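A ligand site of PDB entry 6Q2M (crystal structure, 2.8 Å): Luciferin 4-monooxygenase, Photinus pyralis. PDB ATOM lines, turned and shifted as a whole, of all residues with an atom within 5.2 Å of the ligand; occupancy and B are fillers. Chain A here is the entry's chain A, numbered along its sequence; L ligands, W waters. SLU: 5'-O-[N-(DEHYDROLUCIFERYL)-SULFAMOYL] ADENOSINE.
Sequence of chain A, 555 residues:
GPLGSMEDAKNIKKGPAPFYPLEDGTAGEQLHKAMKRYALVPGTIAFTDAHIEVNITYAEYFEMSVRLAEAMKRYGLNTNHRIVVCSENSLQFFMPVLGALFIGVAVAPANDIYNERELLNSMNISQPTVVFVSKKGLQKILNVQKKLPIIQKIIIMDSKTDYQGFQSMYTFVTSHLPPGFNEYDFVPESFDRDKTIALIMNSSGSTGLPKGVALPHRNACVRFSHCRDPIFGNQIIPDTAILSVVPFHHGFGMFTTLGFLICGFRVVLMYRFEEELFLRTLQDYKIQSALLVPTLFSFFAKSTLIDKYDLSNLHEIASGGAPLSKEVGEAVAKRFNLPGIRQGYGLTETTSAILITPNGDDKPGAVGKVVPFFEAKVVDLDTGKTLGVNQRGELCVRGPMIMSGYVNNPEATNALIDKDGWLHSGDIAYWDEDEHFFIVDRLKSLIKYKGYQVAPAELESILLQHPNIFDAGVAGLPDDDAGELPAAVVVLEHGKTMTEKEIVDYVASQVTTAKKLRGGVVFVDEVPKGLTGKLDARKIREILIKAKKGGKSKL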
ATOM      1  N   SER A 204     -27.221 -25.844  16.019  1.00  0.00           N
ATOM      2  CA  SER A 204     -27.449 -24.535  16.567  1.00  0.00           C
ATOM      3  C   SER A 204     -26.222 -23.663  16.793  1.00  0.00           C
ATOM      4  O   SER A 204     -25.130 -24.108  16.664  1.00  0.00           O
ATOM      5  CB  SER A 204     -28.082 -24.760  17.938  1.00  0.00           C
ATOM      6  OG  SER A 204     -28.972 -25.874  17.974  1.00  0.00           O
ATOM      7  N   ARG A 223     -27.921 -43.743  24.715  1.00  0.00           N
ATOM      8  CA  ARG A 223     -28.732 -42.900  25.584  1.00  0.00           C
ATOM      9  C   ARG A 223     -29.639 -43.731  26.472  1.00  0.00           C
ATOM     10  O   ARG A 223     -29.783 -43.439  27.670  1.00  0.00           O
ATOM     11  CB  ARG A 223     -29.573 -41.922  24.757  1.00  0.00           C
ATOM     12  CG  ARG A 223     -30.596 -41.154  25.588  1.00  0.00           C
ATOM     13  CD  ARG A 223     -29.939 -40.292  26.656  1.00  0.00           C
ATOM     14  NE  ARG A 223     -30.900 -39.763  27.609  1.00  0.00           N
ATOM     15  CZ  ARG A 223     -30.563 -39.225  28.777  1.00  0.00           C
ATOM     16  NH1 ARG A 223     -29.279 -39.164  29.127  1.00  0.00           N
ATOM     17  NH2 ARG A 223     -31.499 -38.769  29.613  1.00  0.00           N
ATOM     18  N   HIS A 250     -35.586 -30.314  19.742  1.00  0.00           N
ATOM     19  CA  HIS A 250     -34.199 -30.127  20.137  1.00  0.00           C
ATOM     20  C   HIS A 250     -33.695 -31.375  20.856  1.00  0.00           C
ATOM     21  O   HIS A 250     -34.469 -32.090  21.497  1.00  0.00           O
ATOM     22  CB  HIS A 250     -34.075 -28.896  21.028  1.00  0.00           C
ATOM     23  CG  HIS A 250     -32.677 -28.538  21.414  1.00  0.00           C
ATOM     24  ND1 HIS A 250     -32.050 -29.043  22.541  1.00  0.00           N
ATOM     25  CD2 HIS A 250     -31.779 -27.698  20.838  1.00  0.00           C
ATOM     26  CE1 HIS A 250     -30.831 -28.542  22.633  1.00  0.00           C
ATOM     27  NE2 HIS A 250     -30.641 -27.734  21.608  1.00  0.00           N
ATOM     28  N   GLY A 251     -32.401 -31.652  20.732  1.00  0.00           N
ATOM     29  CA  GLY A 251     -31.854 -32.888  21.260  1.00  0.00           C
ATOM     30  C   GLY A 251     -32.102 -33.055  22.742  1.00  0.00           C
ATOM     31  O   GLY A 251     -32.285 -34.178  23.234  1.00  0.00           O
ATOM     32  N   PHE A 252     -32.155 -31.931  23.472  1.00  0.00           N
ATOM     33  CA  PHE A 252     -32.383 -31.965  24.912  1.00  0.00           C
ATOM     34  C   PHE A 252     -33.807 -32.411  25.243  1.00  0.00           C
ATOM     35  O   PHE A 252     -34.008 -33.117  26.235  1.00  0.00           O
ATOM     36  CB  PHE A 252     -32.089 -30.574  25.488  1.00  0.00           C
ATOM     37  CG  PHE A 252     -32.375 -30.429  26.952  1.00  0.00           C
ATOM     38  CD1 PHE A 252     -32.304 -31.511  27.818  1.00  0.00           C
ATOM     39  CD2 PHE A 252     -32.563 -29.161  27.496  1.00  0.00           C
ATOM     40  CE1 PHE A 252     -32.514 -31.370  29.179  1.00  0.00           C
ATOM     41  CE2 PHE A 252     -32.763 -29.000  28.868  1.00  0.00           C
ATOM     42  CZ  PHE A 252     -32.743 -30.110  29.714  1.00  0.00           C
ATOM     43  N   THR A 256     -34.114 -36.844  26.226  1.00  0.00           N
ATOM     44  CA  THR A 256     -34.689 -37.017  27.549  1.00  0.00           C
ATOM     45  C   THR A 256     -36.089 -37.646  27.465  1.00  0.00           C
ATOM     46  O   THR A 256     -36.391 -38.584  28.204  1.00  0.00           O
ATOM     47  CB  THR A 256     -34.750 -35.693  28.283  1.00  0.00           C
ATOM     48  OG1 THR A 256     -35.509 -34.759  27.510  1.00  0.00           O
ATOM     49  CG2 THR A 256     -33.334 -35.156  28.550  1.00  0.00           C
ATOM     50  N   LEU A 291     -37.685 -30.958  34.696  1.00  0.00           N
ATOM     51  CA  LEU A 291     -36.617 -30.776  33.738  1.00  0.00           C
ATOM     52  C   LEU A 291     -36.799 -29.444  33.043  1.00  0.00           C
ATOM     53  O   LEU A 291     -37.822 -29.217  32.382  1.00  0.00           O
ATOM     54  CB  LEU A 291     -36.604 -31.932  32.736  1.00  0.00           C
ATOM     55  CG  LEU A 291     -35.522 -31.972  31.662  1.00  0.00           C
ATOM     56  CD1 LEU A 291     -34.120 -32.071  32.278  1.00  0.00           C
ATOM     57  CD2 LEU A 291     -35.788 -33.138  30.720  1.00  0.00           C
ATOM     58  N   ALA A 318     -33.710 -30.580  37.439  1.00  0.00           N
ATOM     59  CA  ALA A 318     -32.614 -30.720  36.498  1.00  0.00           C
ATOM     60  C   ALA A 318     -32.679 -29.579  35.495  1.00  0.00           C
ATOM     61  O   ALA A 318     -33.767 -29.082  35.156  1.00  0.00           O
ATOM     62  CB  ALA A 318     -32.684 -32.073  35.767  1.00  0.00           C
ATOM     63  N   SER A 319     -31.522 -29.170  35.011  1.00  0.00           N
ATOM     64  CA  SER A 319     -31.437 -28.102  34.027  1.00  0.00           C
ATOM     65  C   SER A 319     -30.449 -28.492  32.943  1.00  0.00           C
ATOM     66  O   SER A 319     -29.570 -29.337  33.135  1.00  0.00           O
ATOM     67  CB  SER A 319     -31.011 -26.777  34.664  1.00  0.00           C
ATOM     68  OG  SER A 319     -30.877 -25.769  33.674  1.00  0.00           O
ATOM     69  N   GLY A 320     -30.595 -27.860  31.787  1.00  0.00           N
ATOM     70  CA  GLY A 320     -29.655 -28.151  30.731  1.00  0.00           C
ATOM     71  C   GLY A 320     -29.767 -27.171  29.598  1.00  0.00           C
ATOM     72  O   GLY A 320     -30.608 -26.260  29.610  1.00  0.00           O
ATOM     73  N   GLY A 321     -28.863 -27.326  28.613  1.00  0.00           N
ATOM     74  CA  GLY A 321     -28.910 -26.562  27.393  1.00  0.00           C
ATOM     75  C   GLY A 321     -28.225 -25.208  27.410  1.00  0.00           C
ATOM     76  O   GLY A 321     -28.038 -24.607  26.341  1.00  0.00           O
ATOM     77  N   ALA A 322     -27.848 -24.690  28.586  1.00  0.00           N
ATOM     78  CA  ALA A 322     -27.172 -23.400  28.659  1.00  0.00           C
ATOM     79  C   ALA A 322     -26.610 -23.211  30.057  1.00  0.00           C
ATOM     80  O   ALA A 322     -26.934 -23.980  30.969  1.00  0.00           O
ATOM     81  CB  ALA A 322     -28.115 -22.252  28.300  1.00  0.00           C
ATOM     82  N   PRO A 323     -25.771 -22.204  30.276  1.00  0.00           N
ATOM     83  CA  PRO A 323     -25.221 -21.980  31.616  1.00  0.00           C
ATOM     84  C   PRO A 323     -26.332 -21.673  32.618  1.00  0.00           C
ATOM     85  O   PRO A 323     -27.277 -20.930  32.311  1.00  0.00           O
ATOM     86  CB  PRO A 323     -24.305 -20.765  31.425  1.00  0.00           C
ATOM     87  CG  PRO A 323     -23.996 -20.743  30.001  1.00  0.00           C
ATOM     88  CD  PRO A 323     -25.217 -21.262  29.297  1.00  0.00           C
ATOM     89  N   LEU A 324     -26.235 -22.275  33.798  1.00  0.00           N
ATOM     90  CA  LEU A 324     -27.072 -21.910  34.925  1.00  0.00           C
ATOM     91  C   LEU A 324     -26.198 -21.229  35.954  1.00  0.00           C
ATOM     92  O   LEU A 324     -25.178 -21.790  36.361  1.00  0.00           O
ATOM     93  CB  LEU A 324     -27.772 -23.126  35.529  1.00  0.00           C
ATOM     94  CG  LEU A 324     -28.708 -22.813  36.707  1.00  0.00           C
ATOM     95  CD1 LEU A 324     -29.836 -21.916  36.246  1.00  0.00           C
ATOM     96  CD2 LEU A 324     -29.258 -24.081  37.332  1.00  0.00           C
ATOM     97  N   ARG A 342     -29.524 -30.629  39.193  1.00  0.00           N
ATOM     98  CA  ARG A 342     -28.802 -31.595  38.380  1.00  0.00           C
ATOM     99  C   ARG A 342     -28.526 -31.034  36.994  1.00  0.00           C
ATOM    100  O   ARG A 342     -29.393 -30.420  36.375  1.00  0.00           O
ATOM    101  CB  ARG A 342     -29.579 -32.911  38.268  1.00  0.00           C
ATOM    102  CG  ARG A 342     -28.732 -34.001  37.622  1.00  0.00           C
ATOM    103  CD  ARG A 342     -29.458 -35.320  37.548  1.00  0.00           C
ATOM    104  NE  ARG A 342     -28.545 -36.442  37.369  1.00  0.00           N
ATOM    105  CZ  ARG A 342     -28.941 -37.704  37.278  1.00  0.00           C
ATOM    106  NH1 ARG A 342     -30.222 -38.014  37.352  1.00  0.00           N
ATOM    107  NH2 ARG A 342     -28.045 -38.666  37.120  1.00  0.00           N
ATOM    108  N   GLN A 343     -27.305 -31.246  36.505  1.00  0.00           N
ATOM    109  CA  GLN A 343     -26.875 -30.675  35.245  1.00  0.00           C
ATOM    110  C   GLN A 343     -26.612 -31.761  34.209  1.00  0.00           C
ATOM    111  O   GLN A 343     -26.292 -32.909  34.531  1.00  0.00           O
ATOM    112  CB  GLN A 343     -25.590 -29.840  35.417  1.00  0.00           C
ATOM    113  CG  GLN A 343     -25.774 -28.488  36.057  1.00  0.00           C
ATOM    114  CD  GLN A 343     -26.556 -27.528  35.187  1.00  0.00           C
ATOM    115  OE1 GLN A 343     -26.542 -27.625  33.956  1.00  0.00           O
ATOM    116  NE2 GLN A 343     -27.244 -26.581  35.837  1.00  0.00           N
ATOM    117  N   GLY A 344     -26.774 -31.373  32.948  1.00  0.00           N
ATOM    118  CA  GLY A 344     -26.383 -32.183  31.815  1.00  0.00           C
ATOM    119  C   GLY A 344     -25.852 -31.275  30.735  1.00  0.00           C
ATOM    120  O   GLY A 344     -26.465 -30.263  30.404  1.00  0.00           O
ATOM    121  N   TYR A 345     -24.705 -31.622  30.180  1.00  0.00           N
ATOM    122  CA  TYR A 345     -24.056 -30.876  29.104  1.00  0.00           C
ATOM    123  C   TYR A 345     -23.979 -31.745  27.869  1.00  0.00           C
ATOM    124  O   TYR A 345     -23.557 -32.909  27.955  1.00  0.00           O
ATOM    125  CB  TYR A 345     -22.656 -30.459  29.514  1.00  0.00           C
ATOM    126  CG  TYR A 345     -21.811 -29.932  28.387  1.00  0.00           C
ATOM    127  CD1 TYR A 345     -21.811 -28.585  28.037  1.00  0.00           C
ATOM    128  CD2 TYR A 345     -21.046 -30.793  27.639  1.00  0.00           C
ATOM    129  CE1 TYR A 345     -21.034 -28.123  26.988  1.00  0.00           C
ATOM    130  CE2 TYR A 345     -20.269 -30.350  26.589  1.00  0.00           C
ATOM    131  CZ  TYR A 345     -20.258 -29.006  26.268  1.00  0.00           C
ATOM    132  OH  TYR A 345     -19.461 -28.574  25.217  1.00  0.00           O
ATOM    133  N   GLY A 346     -24.385 -31.202  26.727  1.00  0.00           N
ATOM    134  CA  GLY A 346     -24.297 -31.910  25.472  1.00  0.00           C
ATOM    135  C   GLY A 346     -24.379 -30.930  24.328  1.00  0.00           C
ATOM    136  O   GLY A 346     -24.631 -29.736  24.508  1.00  0.00           O
ATOM    137  N   LEU A 347     -24.127 -31.453  23.130  1.00  0.00           N
ATOM    138  CA  LEU A 347     -24.356 -30.744  21.872  1.00  0.00           C
ATOM    139  C   LEU A 347     -25.295 -31.567  21.007  1.00  0.00           C
ATOM    140  O   LEU A 347     -25.392 -32.798  21.158  1.00  0.00           O
ATOM    141  CB  LEU A 347     -23.060 -30.497  21.101  1.00  0.00           C
ATOM    142  CG  LEU A 347     -21.939 -29.640  21.711  1.00  0.00           C
ATOM    143  CD1 LEU A 347     -21.370 -30.262  22.953  1.00  0.00           C
ATOM    144  CD2 LEU A 347     -20.853 -29.423  20.685  1.00  0.00           C
ATOM    145  N   THR A 348     -25.963 -30.903  20.063  1.00  0.00           N
ATOM    146  CA  THR A 348     -26.795 -31.653  19.139  1.00  0.00           C
ATOM    147  C   THR A 348     -25.968 -32.772  18.502  1.00  0.00           C
ATOM    148  O   THR A 348     -26.488 -33.862  18.256  1.00  0.00           O
ATOM    149  CB  THR A 348     -27.336 -30.750  18.036  1.00  0.00           C
ATOM    150  OG1 THR A 348     -28.034 -29.659  18.636  1.00  0.00           O
ATOM    151  CG2 THR A 348     -28.286 -31.530  17.144  1.00  0.00           C
ATOM    152  N   GLU A 349     -24.672 -32.502  18.274  1.00  0.00           N
ATOM    153  CA  GLU A 349     -23.754 -33.421  17.617  1.00  0.00           C
ATOM    154  C   GLU A 349     -23.314 -34.578  18.496  1.00  0.00           C
ATOM    155  O   GLU A 349     -22.751 -35.542  17.969  1.00  0.00           O
ATOM    156  CB  GLU A 349     -22.523 -32.652  17.145  1.00  0.00           C
ATOM    157  CG  GLU A 349     -22.745 -31.640  15.998  1.00  0.00           C
ATOM    158  CD  GLU A 349     -23.246 -30.250  16.441  1.00  0.00           C
ATOM    159  OE1 GLU A 349     -23.541 -30.068  17.647  1.00  0.00           O
ATOM    160  OE2 GLU A 349     -23.298 -29.330  15.593  1.00  0.00           O
ATOM    161  N   THR A 351     -25.639 -36.117  20.469  1.00  0.00           N
ATOM    162  CA  THR A 351     -26.939 -36.765  20.652  1.00  0.00           C
ATOM    163  C   THR A 351     -27.630 -36.271  21.914  1.00  0.00           C
ATOM    164  O   THR A 351     -28.788 -35.853  21.873  1.00  0.00           O
ATOM    165  CB  THR A 351     -26.820 -38.297  20.754  1.00  0.00           C
ATOM    166  OG1 THR A 351     -26.116 -38.841  19.629  1.00  0.00           O
ATOM    167  CG2 THR A 351     -28.225 -38.926  20.821  1.00  0.00           C
ATOM    168  N   SER A 352     -26.899 -36.224  23.024  1.00  0.00           N
ATOM    169  CA  SER A 352     -27.490 -35.974  24.326  1.00  0.00           C
ATOM    170  C   SER A 352     -26.371 -35.570  25.266  1.00  0.00           C
ATOM    171  O   SER A 352     -25.244 -35.324  24.832  1.00  0.00           O
ATOM    172  CB  SER A 352     -28.254 -37.211  24.820  1.00  0.00           C
ATOM    173  OG  SER A 352     -28.939 -36.954  26.035  1.00  0.00           O
ATOM    174  N   ALA A 353     -26.704 -35.452  26.550  1.00  0.00           N
ATOM    175  CA  ALA A 353     -25.714 -35.081  27.553  1.00  0.00           C
ATOM    176  C   ALA A 353     -24.610 -36.133  27.643  1.00  0.00           C
ATOM    177  O   ALA A 353     -24.871 -37.301  27.924  1.00  0.00           O
ATOM    178  CB  ALA A 353     -26.383 -34.894  28.913  1.00  0.00           C
ATOM    179  N   VAL A 367     -21.015 -29.153  35.562  1.00  0.00           N
ATOM    180  CA  VAL A 367     -22.031 -29.797  34.742  1.00  0.00           C
ATOM    181  C   VAL A 367     -21.973 -31.307  34.828  1.00  0.00           C
ATOM    182  O   VAL A 367     -22.725 -31.982  34.117  1.00  0.00           O
ATOM    183  CB  VAL A 367     -21.949 -29.309  33.288  1.00  0.00           C
ATOM    184  CG1 VAL A 367     -22.277 -27.817  33.221  1.00  0.00           C
ATOM    185  CG2 VAL A 367     -20.551 -29.578  32.709  1.00  0.00           C
ATOM    186  N   SER A 425     -15.713 -29.265  20.835  1.00  0.00           N
ATOM    187  CA  SER A 425     -17.014 -28.735  21.238  1.00  0.00           C
ATOM    188  C   SER A 425     -17.170 -27.251  20.953  1.00  0.00           C
ATOM    189  O   SER A 425     -18.301 -26.777  20.824  1.00  0.00           O
ATOM    190  CB  SER A 425     -17.233 -28.963  22.724  1.00  0.00           C
ATOM    191  OG  SER A 425     -16.298 -28.183  23.466  1.00  0.00           O
ATOM    192  N   ASP A 427     -16.247 -25.131  23.241  1.00  0.00           N
ATOM    193  CA  ASP A 427     -16.463 -24.608  24.588  1.00  0.00           C
ATOM    194  C   ASP A 427     -15.154 -24.627  25.382  1.00  0.00           C
ATOM    195  O   ASP A 427     -14.348 -25.549  25.231  1.00  0.00           O
ATOM    196  CB  ASP A 427     -17.525 -25.417  25.332  1.00  0.00           C
ATOM    197  CG  ASP A 427     -18.923 -25.193  24.785  1.00  0.00           C
ATOM    198  OD1 ASP A 427     -19.227 -24.060  24.392  1.00  0.00           O
ATOM    199  OD2 ASP A 427     -19.725 -26.163  24.748  1.00  0.00           O
ATOM    200  N   ILE A 439     -17.954 -25.665  32.632  1.00  0.00           N
ATOM    201  CA  ILE A 439     -17.994 -24.976  31.347  1.00  0.00           C
ATOM    202  C   ILE A 439     -17.791 -23.501  31.590  1.00  0.00           C
ATOM    203  O   ILE A 439     -18.548 -22.892  32.350  1.00  0.00           O
ATOM    204  CB  ILE A 439     -19.324 -25.211  30.615  1.00  0.00           C
ATOM    205  CG1 ILE A 439     -19.596 -26.697  30.404  1.00  0.00           C
ATOM    206  CG2 ILE A 439     -19.304 -24.480  29.290  1.00  0.00           C
ATOM    207  CD1 ILE A 439     -18.574 -27.401  29.517  1.00  0.00           C
ATOM    208  N   ARG A 442     -18.233 -19.955  25.609  1.00  0.00           N
ATOM    209  CA  ARG A 442     -18.146 -20.385  24.252  1.00  0.00           C
ATOM    210  C   ARG A 442     -16.857 -19.806  23.755  1.00  0.00           C
ATOM    211  O   ARG A 442     -16.526 -18.717  24.048  1.00  0.00           O
ATOM    212  CB  ARG A 442     -19.346 -19.843  23.569  1.00  0.00           C
ATOM    213  CG  ARG A 442     -19.630 -20.350  22.221  1.00  0.00           C
ATOM    214  CD  ARG A 442     -20.324 -21.693  22.185  1.00  0.00           C
ATOM    215  NE  ARG A 442     -20.067 -22.237  20.855  1.00  0.00           N
ATOM    216  CZ  ARG A 442     -20.002 -23.498  20.516  1.00  0.00           C
ATOM    217  NH1 ARG A 442     -20.229 -24.427  21.394  1.00  0.00           N
ATOM    218  NH2 ARG A 442     -19.729 -23.799  19.282  1.00  0.00           N
ATOM    219  N   THR A 532     -33.343 -22.678  24.404  1.00  0.00           N
ATOM    220  CA  THR A 532     -32.773 -23.198  25.632  1.00  0.00           C
ATOM    221  C   THR A 532     -32.083 -22.120  26.453  1.00  0.00           C
ATOM    222  O   THR A 532     -31.556 -22.409  27.528  1.00  0.00           O
ATOM    223  CB  THR A 532     -31.775 -24.322  25.320  1.00  0.00           C
ATOM    224  OG1 THR A 532     -30.739 -23.816  24.475  1.00  0.00           O
ATOM    225  CG2 THR A 532     -32.482 -25.489  24.614  1.00  0.00           C
ATOM    226  N   LYS A 534     -29.447 -19.845  25.401  1.00  0.00           N
ATOM    227  CA  LYS A 534     -28.113 -19.359  25.086  1.00  0.00           C
ATOM    228  C   LYS A 534     -28.206 -17.911  24.596  1.00  0.00           C
ATOM    229  O   LYS A 534     -29.120 -17.559  23.850  1.00  0.00           O
ATOM    230  CB  LYS A 534     -27.440 -20.226  24.000  1.00  0.00           C
ATOM    231  CG  LYS A 534     -27.445 -21.736  24.249  1.00  0.00           C
ATOM    232  CD  LYS A 534     -27.149 -22.493  22.943  1.00  0.00           C
ATOM    233  CE  LYS A 534     -27.057 -24.022  23.147  1.00  0.00           C
ATOM    234  NZ  LYS A 534     -28.327 -24.700  23.617  1.00  0.00           N
HETATM  235  O39 SLU L   1     -27.791 -28.039  23.843  1.00  0.00           O
HETATM  236  C16 SLU L   1     -27.652 -28.992  23.232  1.00  0.00           C
HETATM  237  C14 SLU L   1     -28.024 -30.331  23.826  1.00  0.00           C
HETATM  238  N15 SLU L   1     -28.233 -30.436  25.280  1.00  0.00           N
HETATM  239  C13 SLU L   1     -28.219 -31.578  23.186  1.00  0.00           C
HETATM  240  S12 SLU L   1     -28.519 -32.469  24.259  1.00  0.00           S
HETATM  241  C11 SLU L   1     -28.515 -31.724  25.554  1.00  0.00           C
HETATM  242  C8  SLU L   1     -28.780 -31.992  26.889  1.00  0.00           C
HETATM  243  S9  SLU L   1     -28.757 -31.216  28.154  1.00  0.00           S
HETATM  244  C4  SLU L   1     -29.270 -32.150  29.162  1.00  0.00           C
HETATM  245  C5  SLU L   1     -29.441 -32.007  30.492  1.00  0.00           C
HETATM  246  C6  SLU L   1     -29.925 -33.043  31.221  1.00  0.00           C
HETATM  247  O10 SLU L   1     -30.147 -33.060  32.561  1.00  0.00           O
HETATM  248  C3  SLU L   1     -29.583 -33.359  28.569  1.00  0.00           C
HETATM  249  N7  SLU L   1     -29.295 -33.242  27.083  1.00  0.00           N
HETATM  250  C2  SLU L   1     -30.057 -34.385  29.299  1.00  0.00           C
HETATM  251  C1  SLU L   1     -30.227 -34.222  30.640  1.00  0.00           C
HETATM  252  N40 SLU L   1     -27.119 -28.980  21.920  1.00  0.00           N
HETATM  253  S17 SLU L   1     -26.785 -27.441  21.340  1.00  0.00           S
HETATM  254  O18 SLU L   1     -27.957 -26.708  21.382  1.00  0.00           O
HETATM  255  O19 SLU L   1     -26.683 -27.331  19.980  1.00  0.00           O
HETATM  256  O20 SLU L   1     -25.613 -26.556  21.971  1.00  0.00           O
HETATM  257  C21 SLU L   1     -24.636 -26.995  22.809  1.00  0.00           C
HETATM  258  C22 SLU L   1     -24.319 -25.712  23.497  1.00  0.00           C
HETATM  259  C23 SLU L   1     -23.104 -26.089  24.251  1.00  0.00           C
HETATM  260  O27 SLU L   1     -21.988 -25.995  23.556  1.00  0.00           O
HETATM  261  C24 SLU L   1     -23.046 -25.120  25.337  1.00  0.00           C
HETATM  262  O28 SLU L   1     -22.569 -23.813  24.888  1.00  0.00           O
HETATM  263  C25 SLU L   1     -24.394 -25.088  25.688  1.00  0.00           C
HETATM  264  O26 SLU L   1     -25.198 -25.514  24.575  1.00  0.00           O
HETATM  265  N35 SLU L   1     -24.657 -25.787  26.884  1.00  0.00           N
HETATM  266  C32 SLU L   1     -24.411 -25.665  28.147  1.00  0.00           C
HETATM  267  N31 SLU L   1     -23.755 -24.791  28.895  1.00  0.00           N
HETATM  268  C30 SLU L   1     -23.689 -24.950  30.196  1.00  0.00           C
HETATM  269  N29 SLU L   1     -24.289 -25.983  30.759  1.00  0.00           N
HETATM  270  C33 SLU L   1     -24.991 -26.698  28.709  1.00  0.00           C
HETATM  271  C34 SLU L   1     -24.913 -26.850  30.060  1.00  0.00           C
HETATM  272  N38 SLU L   1     -25.512 -27.927  30.680  1.00  0.00           N
HETATM  273  N37 SLU L   1     -25.552 -27.419  27.757  1.00  0.00           N
HETATM  274  C36 SLU L   1     -25.337 -26.844  26.625  1.00  0.00           C
HETATM  275  O   HOH W   1     -30.834 -35.229  25.468  1.00  0.00           O
HETATM  276  O   HOH W   2     -22.013 -22.306  27.408  1.00  0.00           O
HETATM  277  O   HOH W   3     -25.960 -27.459  17.298  1.00  0.00           O
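O of Gly 344 is in hydrogen-bond range of N38 of the ligand. OD2 of Asp 427 lies within hydrogen-bond range of O27 of the ligand (2.6 Å). The side-chain amino group of Lys 534 sits at hydrogen-bond distance from an oxygen (O18) of the ligand (3.0 Å). A ring nitrogen (NE2) of His 250 lies within hydrogen-bond range of an oxygen (O18) of the ligand. The backbone NH (N) of Thr 348 is in hydrogen-bond range of a nitrogen (N40) of the ligand, at 2.9 Å. The side-chain hydroxyl of Thr 348 lies within hydrogen-bond range of an oxygen (O19) of the ligand (3.0 Å). NH1 of Arg 442 sits at hydrogen-bond distance from O27 of the ligand, 3.2 Å away. N of Phe 252 sits close to S12 of the ligand, at 3.8 Å. An oxygen (O19) of the ligand lies within hydrogen-bond range of the side-chain hydroxyl (OG) of Ser 204 (3.4 Å). N of Gly 321 sits at hydrogen-bond distance from N37 of the ligand. N7 of the ligand lies within hydrogen-bond range of N of Ala 353, 3.4 Å away. The side-chain amide oxygen (OE1) of Gln 343 lies within hydrogen-bond range of a nitrogen (N38) of the ligand (3.4 Å).
The backbone NH (N) of Gly 344 lies within hydrogen-bond range of the backbone carbonyl oxygen (O) of Ser 319. The guanidinium group (NH1) of Arg 442 lies within salt-bridge range of the side-chain carboxylate (OD1) of Asp 427 (3.2 Å). The side-chain carboxylate (OD2) of Asp 427 sits at hydrogen-bond distance from the side-chain hydroxyl (OH) of Tyr 345. The side-chain amino group (NZ) of Lys 534 is in hydrogen-bond range of the backbone carbonyl oxygen (O) of Gly 321, 2.7 Å away. NZ of Lys 534 lies within hydrogen-bond range of OG1 of Thr 532, at 2.7 Å. O of Ser 425 sits at hydrogen-bond distance from NH1 of Arg 442, at 3.1 Å. O of Gly 321 is in hydrogen-bond range of OG1 of Thr 532 (3.4 Å). The backbone carbonyl oxygen (O) of Arg 342 sits at hydrogen-bond distance from the backbone NH (N) of Ser 319 (2.8 Å).
The backbone carbonyl oxygen (O) of Ala 322 sits close to a nitrogen (N29) of the ligand. Merely in contact with the ligand: Gly 251 (3.9 Å), Thr 256 (3.4 Å), Ser 319 (3.8 Å), Gly 320 (3.9 Å), Pro 323 (3.4 Å), Tyr 345 (3.6 Å), Gly 346 (3.2 Å), Leu 347 (3.3 Å), Ser 352 (3.7 Å) and Val 367 (3.7 Å). Hydrophobic or aromatic side chains that line the ligand: His 250, Phe 252, Pro 323, Tyr 345, Leu 347, Ala 353 and Val 367. The nearest printed residue that does not touch the ligand is Leu 291 (4.1 Å).
Water W3 lies within hydrogen-bond range of the backbone NH (N) of Ser 204 (2.4 Å), an oxygen (O19) of the ligand (2.8 Å) and the side-chain hydroxyl (OG1) of Thr 348 (3.3 Å). Water W1 lies within hydrogen-bond range of OG of Ser 352 (2.6 Å), O of Gly 251 (2.9 Å) and N7 of the ligand (3.0 Å).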
